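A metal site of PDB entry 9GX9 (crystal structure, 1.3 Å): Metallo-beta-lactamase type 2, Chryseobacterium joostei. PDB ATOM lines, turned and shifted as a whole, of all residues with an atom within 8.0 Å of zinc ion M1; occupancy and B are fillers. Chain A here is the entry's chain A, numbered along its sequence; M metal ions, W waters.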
ATOM      1  N   LYS A  38      25.109   7.821  -0.959  1.00  0.00           N
ATOM      2  CA  LYS A  38      24.161   6.925  -0.318  1.00  0.00           C
ATOM      3  C   LYS A  38      24.024   7.337   1.135  1.00  0.00           C
ATOM      4  O   LYS A  38      25.029   7.467   1.849  1.00  0.00           O
ATOM      5  CB  LYS A  38      24.679   5.494  -0.399  1.00  0.00           C
ATOM      6  CG  LYS A  38      23.832   4.448   0.302  1.00  0.00           C
ATOM      7  CD  LYS A  38      24.324   3.049  -0.054  1.00  0.00           C
ATOM      8  CE  LYS A  38      24.128   2.070   1.107  1.00  0.00           C
ATOM      9  NZ  LYS A  38      23.165   0.980   0.779  1.00  0.00           N
ATOM     10  N   PRO A  47      30.142   8.292  -0.557  1.00  0.00           N
ATOM     11  CA  PRO A  47      30.169   8.467  -2.014  1.00  0.00           C
ATOM     12  C   PRO A  47      30.148   7.133  -2.750  1.00  0.00           C
ATOM     13  O   PRO A  47      30.666   6.114  -2.279  1.00  0.00           O
ATOM     14  CB  PRO A  47      31.497   9.197  -2.270  1.00  0.00           C
ATOM     15  CG  PRO A  47      32.368   8.779  -1.115  1.00  0.00           C
ATOM     16  CD  PRO A  47      31.435   8.626   0.067  1.00  0.00           C
ATOM     17  N   CYS A  48      29.525   7.181  -3.922  1.00  0.00           N
ATOM     18  CA  CYS A  48      29.300   6.017  -4.769  1.00  0.00           C
ATOM     19  C   CYS A  48      29.590   6.432  -6.211  1.00  0.00           C
ATOM     20  O   CYS A  48      29.113   7.493  -6.633  1.00  0.00           O
ATOM     21  CB  CYS A  48      27.833   5.587  -4.698  1.00  0.00           C
ATOM     22  SG  CYS A  48      27.258   5.135  -3.068  1.00  0.00           S
ATOM     23  N   ASN A  49      30.318   5.599  -6.953  1.00  0.00           N
ATOM     24  CA  ASN A  49      30.758   5.966  -8.296  1.00  0.00           C
ATOM     25  C   ASN A  49      30.036   5.196  -9.406  1.00  0.00           C
ATOM     26  O   ASN A  49      29.653   4.033  -9.243  1.00  0.00           O
ATOM     27  CB  ASN A  49      32.247   5.681  -8.482  1.00  0.00           C
ATOM     28  CG  ASN A  49      33.116   6.483  -7.555  1.00  0.00           C
ATOM     29  OD1 ASN A  49      32.816   7.636  -7.252  1.00  0.00           O
ATOM     30  ND2 ASN A  49      34.186   5.876  -7.085  1.00  0.00           N
ATOM     31  N   ASP A  63      26.135   2.156 -13.860  1.00  0.00           N
ATOM     32  CA  ASP A  63      25.597   2.428 -12.527  1.00  0.00           C
ATOM     33  C   ASP A  63      24.663   3.625 -12.503  1.00  0.00           C
ATOM     34  O   ASP A  63      24.928   4.635 -13.145  1.00  0.00           O
ATOM     35  CB  ASP A  63      26.644   2.562 -11.423  1.00  0.00           C
ATOM     36  CG  ASP A  63      27.155   1.226 -10.916  1.00  0.00           C
ATOM     37  OD1 ASP A  63      26.972   0.185 -11.619  1.00  0.00           O
ATOM     38  OD2 ASP A  63      27.724   1.227  -9.790  1.00  0.00           O
ATOM     39  N   THR A  92      25.863  -2.364 -12.528  1.00  0.00           N
ATOM     40  CA  THR A  92      26.858  -3.426 -12.406  1.00  0.00           C
ATOM     41  C   THR A  92      26.561  -4.423 -11.301  1.00  0.00           C
ATOM     42  O   THR A  92      27.223  -5.471 -11.247  1.00  0.00           O
ATOM     43  CB  THR A  92      28.289  -2.877 -12.251  1.00  0.00           C
ATOM     44  OG1 THR A  92      28.364  -2.049 -11.089  1.00  0.00           O
ATOM     45  CG2 THR A  92      28.657  -2.091 -13.488  1.00  0.00           C
ATOM     46  N   HIS A  93      25.629  -4.119 -10.397  1.00  0.00           N
ATOM     47  CA  HIS A  93      25.100  -5.109  -9.476  1.00  0.00           C
ATOM     48  C   HIS A  93      23.767  -4.604  -8.923  1.00  0.00           C
ATOM     49  O   HIS A  93      23.363  -3.480  -9.213  1.00  0.00           O
ATOM     50  CB  HIS A  93      26.119  -5.536  -8.414  1.00  0.00           C
ATOM     51  CG  HIS A  93      26.372  -4.557  -7.318  1.00  0.00           C
ATOM     52  ND1 HIS A  93      26.742  -3.236  -7.524  1.00  0.00           N
ATOM     53  CD2 HIS A  93      26.409  -4.737  -5.979  1.00  0.00           C
ATOM     54  CE1 HIS A  93      26.974  -2.658  -6.368  1.00  0.00           C
ATOM     55  NE2 HIS A  93      26.776  -3.533  -5.421  1.00  0.00           N
ATOM     56  N   HIS A  95      22.626  -3.962  -5.840  1.00  0.00           N
ATOM     57  CA  HIS A  95      22.512  -3.068  -4.695  1.00  0.00           C
ATOM     58  C   HIS A  95      22.123  -1.661  -5.132  1.00  0.00           C
ATOM     59  O   HIS A  95      22.349  -1.239  -6.283  1.00  0.00           O
ATOM     60  CB  HIS A  95      23.819  -2.996  -3.918  1.00  0.00           C
ATOM     61  CG  HIS A  95      24.151  -4.220  -3.143  1.00  0.00           C
ATOM     62  ND1 HIS A  95      25.415  -4.467  -2.654  1.00  0.00           N
ATOM     63  CD2 HIS A  95      23.388  -5.259  -2.733  1.00  0.00           C
ATOM     64  CE1 HIS A  95      25.414  -5.609  -1.993  1.00  0.00           C
ATOM     65  NE2 HIS A  95      24.197  -6.115  -2.032  1.00  0.00           N
ATOM     66  N   ASP A  96      21.560  -0.899  -4.179  1.00  0.00           N
ATOM     67  CA  ASP A  96      21.064   0.437  -4.506  1.00  0.00           C
ATOM     68  C   ASP A  96      22.136   1.381  -5.043  1.00  0.00           C
ATOM     69  O   ASP A  96      21.810   2.258  -5.850  1.00  0.00           O
ATOM     70  CB  ASP A  96      20.318   1.065  -3.332  1.00  0.00           C
ATOM     71  CG  ASP A  96      21.175   1.269  -2.097  1.00  0.00           C
ATOM     72  OD1 ASP A  96      22.309   0.734  -2.004  1.00  0.00           O
ATOM     73  OD2 ASP A  96      20.683   1.991  -1.202  1.00  0.00           O
ATOM     74  N   ASP A  97      23.398   1.230  -4.648  1.00  0.00           N
ATOM     75  CA  ASP A  97      24.416   2.141  -5.154  1.00  0.00           C
ATOM     76  C   ASP A  97      24.847   1.826  -6.575  1.00  0.00           C
ATOM     77  O   ASP A  97      25.724   2.501  -7.107  1.00  0.00           O
ATOM     78  CB  ASP A  97      25.612   2.223  -4.203  1.00  0.00           C
ATOM     79  CG  ASP A  97      26.244   0.897  -3.930  1.00  0.00           C
ATOM     80  OD1 ASP A  97      25.558  -0.015  -3.420  1.00  0.00           O
ATOM     81  OD2 ASP A  97      27.460   0.756  -4.220  1.00  0.00           O
ATOM     82  N   SER A  98      24.266   0.814  -7.197  1.00  0.00           N
ATOM     83  CA  SER A  98      24.412   0.608  -8.630  1.00  0.00           C
ATOM     84  C   SER A  98      23.108   0.664  -9.392  1.00  0.00           C
ATOM     85  O   SER A  98      23.134   0.863 -10.608  1.00  0.00           O
ATOM     86  CB  SER A  98      25.064  -0.757  -8.943  1.00  0.00           C
ATOM     87  OG  SER A  98      26.427  -0.767  -8.589  1.00  0.00           O
ATOM     88  N   HIS A 156      32.175  -9.198  -4.618  1.00  0.00           N
ATOM     89  CA  HIS A 156      31.372  -8.349  -3.749  1.00  0.00           C
ATOM     90  C   HIS A 156      29.928  -8.818  -3.688  1.00  0.00           C
ATOM     91  O   HIS A 156      29.315  -8.837  -2.613  1.00  0.00           O
ATOM     92  CB  HIS A 156      31.462  -6.932  -4.286  1.00  0.00           C
ATOM     93  CG  HIS A 156      30.521  -6.005  -3.615  1.00  0.00           C
ATOM     94  ND1 HIS A 156      30.724  -5.554  -2.330  1.00  0.00           N
ATOM     95  CD2 HIS A 156      29.352  -5.472  -4.033  1.00  0.00           C
ATOM     96  CE1 HIS A 156      29.723  -4.755  -1.994  1.00  0.00           C
ATOM     97  NE2 HIS A 156      28.881  -4.703  -3.005  1.00  0.00           N
ATOM     98  N   THR A 157      29.381  -9.210  -4.829  1.00  0.00           N
ATOM     99  CA  THR A 157      28.104  -9.911  -4.914  1.00  0.00           C
ATOM    100  C   THR A 157      28.268 -11.024  -5.938  1.00  0.00           C
ATOM    101  O   THR A 157      29.289 -11.137  -6.617  1.00  0.00           O
ATOM    102  CB  THR A 157      26.940  -8.997  -5.319  1.00  0.00           C
ATOM    103  OG1 THR A 157      27.287  -8.353  -6.547  1.00  0.00           O
ATOM    104  CG2 THR A 157      26.636  -7.986  -4.251  1.00  0.00           C
ATOM    105  N   GLY A 174      33.250  -1.244 -10.563  1.00  0.00           N
ATOM    106  CA  GLY A 174      32.141  -1.364  -9.650  1.00  0.00           C
ATOM    107  C   GLY A 174      32.622  -1.766  -8.260  1.00  0.00           C
ATOM    108  O   GLY A 174      33.796  -1.614  -7.892  1.00  0.00           O
ATOM    109  N   CYS A 175      31.693  -2.312  -7.479  1.00  0.00           N
ATOM    110  CA  CYS A 175      32.009  -2.627  -6.089  1.00  0.00           C
ATOM    111  C   CYS A 175      32.862  -3.881  -5.935  1.00  0.00           C
ATOM    112  O   CYS A 175      33.357  -4.159  -4.831  1.00  0.00           O
ATOM    113  CB  CYS A 175      30.705  -2.673  -5.300  1.00  0.00           C
ATOM    114  SG  CYS A 175      29.895  -1.033  -5.384  1.00  0.00           S
ATOM    115  N   LEU A 176      33.111  -4.604  -7.019  1.00  0.00           N
ATOM    116  CA  LEU A 176      34.120  -5.637  -7.043  1.00  0.00           C
ATOM    117  C   LEU A 176      35.517  -5.067  -6.843  1.00  0.00           C
ATOM    118  O   LEU A 176      36.397  -5.768  -6.331  1.00  0.00           O
ATOM    119  CB  LEU A 176      34.060  -6.337  -8.412  1.00  0.00           C
ATOM    120  CG  LEU A 176      35.050  -7.468  -8.681  1.00  0.00           C
ATOM    121  CD1 LEU A 176      34.686  -8.691  -7.835  1.00  0.00           C
ATOM    122  CD2 LEU A 176      35.051  -7.833 -10.157  1.00  0.00           C
ATOM    123  N   LEU A 177      35.732  -3.803  -7.197  1.00  0.00           N
ATOM    124  CA  LEU A 177      37.031  -3.178  -7.056  1.00  0.00           C
ATOM    125  C   LEU A 177      37.034  -2.219  -5.884  1.00  0.00           C
ATOM    126  O   LEU A 177      36.081  -1.441  -5.688  1.00  0.00           O
ATOM    127  CB  LEU A 177      37.391  -2.405  -8.319  1.00  0.00           C
ATOM    128  CG  LEU A 177      38.224  -3.153  -9.362  1.00  0.00           C
ATOM    129  CD1 LEU A 177      39.630  -3.387  -8.860  1.00  0.00           C
ATOM    130  CD2 LEU A 177      37.578  -4.470  -9.788  1.00  0.00           C
ATOM    131  N   LYS A 178      38.110  -2.258  -5.115  1.00  0.00           N
ATOM    132  CA  LYS A 178      38.311  -1.396  -3.957  1.00  0.00           C
ATOM    133  C   LYS A 178      39.345  -0.338  -4.277  1.00  0.00           C
ATOM    134  O   LYS A 178      40.299  -0.554  -5.035  1.00  0.00           O
ATOM    135  CB  LYS A 178      38.784  -2.209  -2.761  1.00  0.00           C
ATOM    136  CG  LYS A 178      37.778  -3.255  -2.247  1.00  0.00           C
ATOM    137  CD  LYS A 178      36.489  -2.654  -1.767  1.00  0.00           C
ATOM    138  CE  LYS A 178      35.600  -3.679  -1.111  1.00  0.00           C
ATOM    139  NZ  LYS A 178      34.340  -3.036  -0.661  1.00  0.00           N
ATOM    140  N   TYR A 186      31.122  -3.955   2.875  1.00  0.00           N
ATOM    141  CA  TYR A 186      29.963  -4.773   3.187  1.00  0.00           C
ATOM    142  C   TYR A 186      30.088  -6.139   2.533  1.00  0.00           C
ATOM    143  O   TYR A 186      30.196  -6.248   1.302  1.00  0.00           O
ATOM    144  CB  TYR A 186      28.700  -4.092   2.697  1.00  0.00           C
ATOM    145  CG  TYR A 186      27.458  -4.921   2.875  1.00  0.00           C
ATOM    146  CD1 TYR A 186      26.851  -5.067   4.128  1.00  0.00           C
ATOM    147  CD2 TYR A 186      26.875  -5.566   1.791  1.00  0.00           C
ATOM    148  CE1 TYR A 186      25.711  -5.821   4.287  1.00  0.00           C
ATOM    149  CE2 TYR A 186      25.735  -6.320   1.950  1.00  0.00           C
ATOM    150  CZ  TYR A 186      25.159  -6.440   3.192  1.00  0.00           C
ATOM    151  OH  TYR A 186      24.032  -7.195   3.326  1.00  0.00           O
ATOM    152  N   PRO A 214      36.878   2.266  -8.766  1.00  0.00           N
ATOM    153  CA  PRO A 214      36.158   1.424  -7.799  1.00  0.00           C
ATOM    154  C   PRO A 214      34.743   1.928  -7.593  1.00  0.00           C
ATOM    155  O   PRO A 214      34.403   3.065  -7.884  1.00  0.00           O
ATOM    156  CB  PRO A 214      36.980   1.605  -6.508  1.00  0.00           C
ATOM    157  CG  PRO A 214      37.417   2.998  -6.584  1.00  0.00           C
ATOM    158  CD  PRO A 214      37.691   3.277  -8.079  1.00  0.00           C
ATOM    159  N   GLY A 215      33.908   1.065  -7.010  1.00  0.00           N
ATOM    160  CA  GLY A 215      32.537   1.460  -6.704  1.00  0.00           C
ATOM    161  C   GLY A 215      32.427   2.578  -5.685  1.00  0.00           C
ATOM    162  O   GLY A 215      31.437   3.339  -5.679  1.00  0.00           O
ATOM    163  N   HIS A 216      33.396   2.669  -4.782  1.00  0.00           N
ATOM    164  CA  HIS A 216      33.450   3.720  -3.773  1.00  0.00           C
ATOM    165  C   HIS A 216      34.877   4.234  -3.679  1.00  0.00           C
ATOM    166  O   HIS A 216      35.833   3.445  -3.605  1.00  0.00           O
ATOM    167  CB  HIS A 216      32.999   3.212  -2.401  1.00  0.00           C
ATOM    168  CG  HIS A 216      31.644   2.595  -2.427  1.00  0.00           C
ATOM    169  ND1 HIS A 216      30.491   3.347  -2.453  1.00  0.00           N
ATOM    170  CD2 HIS A 216      31.255   1.306  -2.509  1.00  0.00           C
ATOM    171  CE1 HIS A 216      29.441   2.541  -2.522  1.00  0.00           C
ATOM    172  NE2 HIS A 216      29.880   1.295  -2.561  1.00  0.00           N
HETATM  173 ZN    ZN M   1      29.097  -0.626  -3.416  1.00  0.00          ZN
HETATM  174 ZN    ZN M   2      27.195  -3.459  -3.334  1.00  0.00          ZN
HETATM  175  O   HOH W   1      27.496  -1.684  -2.724  1.00  0.00           O
HETATM  176  O   HOH W   2      30.551  -1.878  -2.190  1.00  0.00           O
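ND1 of His 216 sits at hydrogen-bond distance from O of Pro 47 (2.8 Å).
SG of Cys 48 sits close to ND1 of His 216.
Of the 22 residues printed, 3 come within 4 Å of zinc ion M1.
The nearest printed residue that does not touch zinc ion M1 is His 156 (4.1 Å).
Zinc ion M1 is bound by water W1 (2.0 Å), SG of Cys 175 (2.2 Å), NE2 of His 216 (2.2 Å), water W2 (2.3 Å) and OD2 of Asp 97 (2.3 Å).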
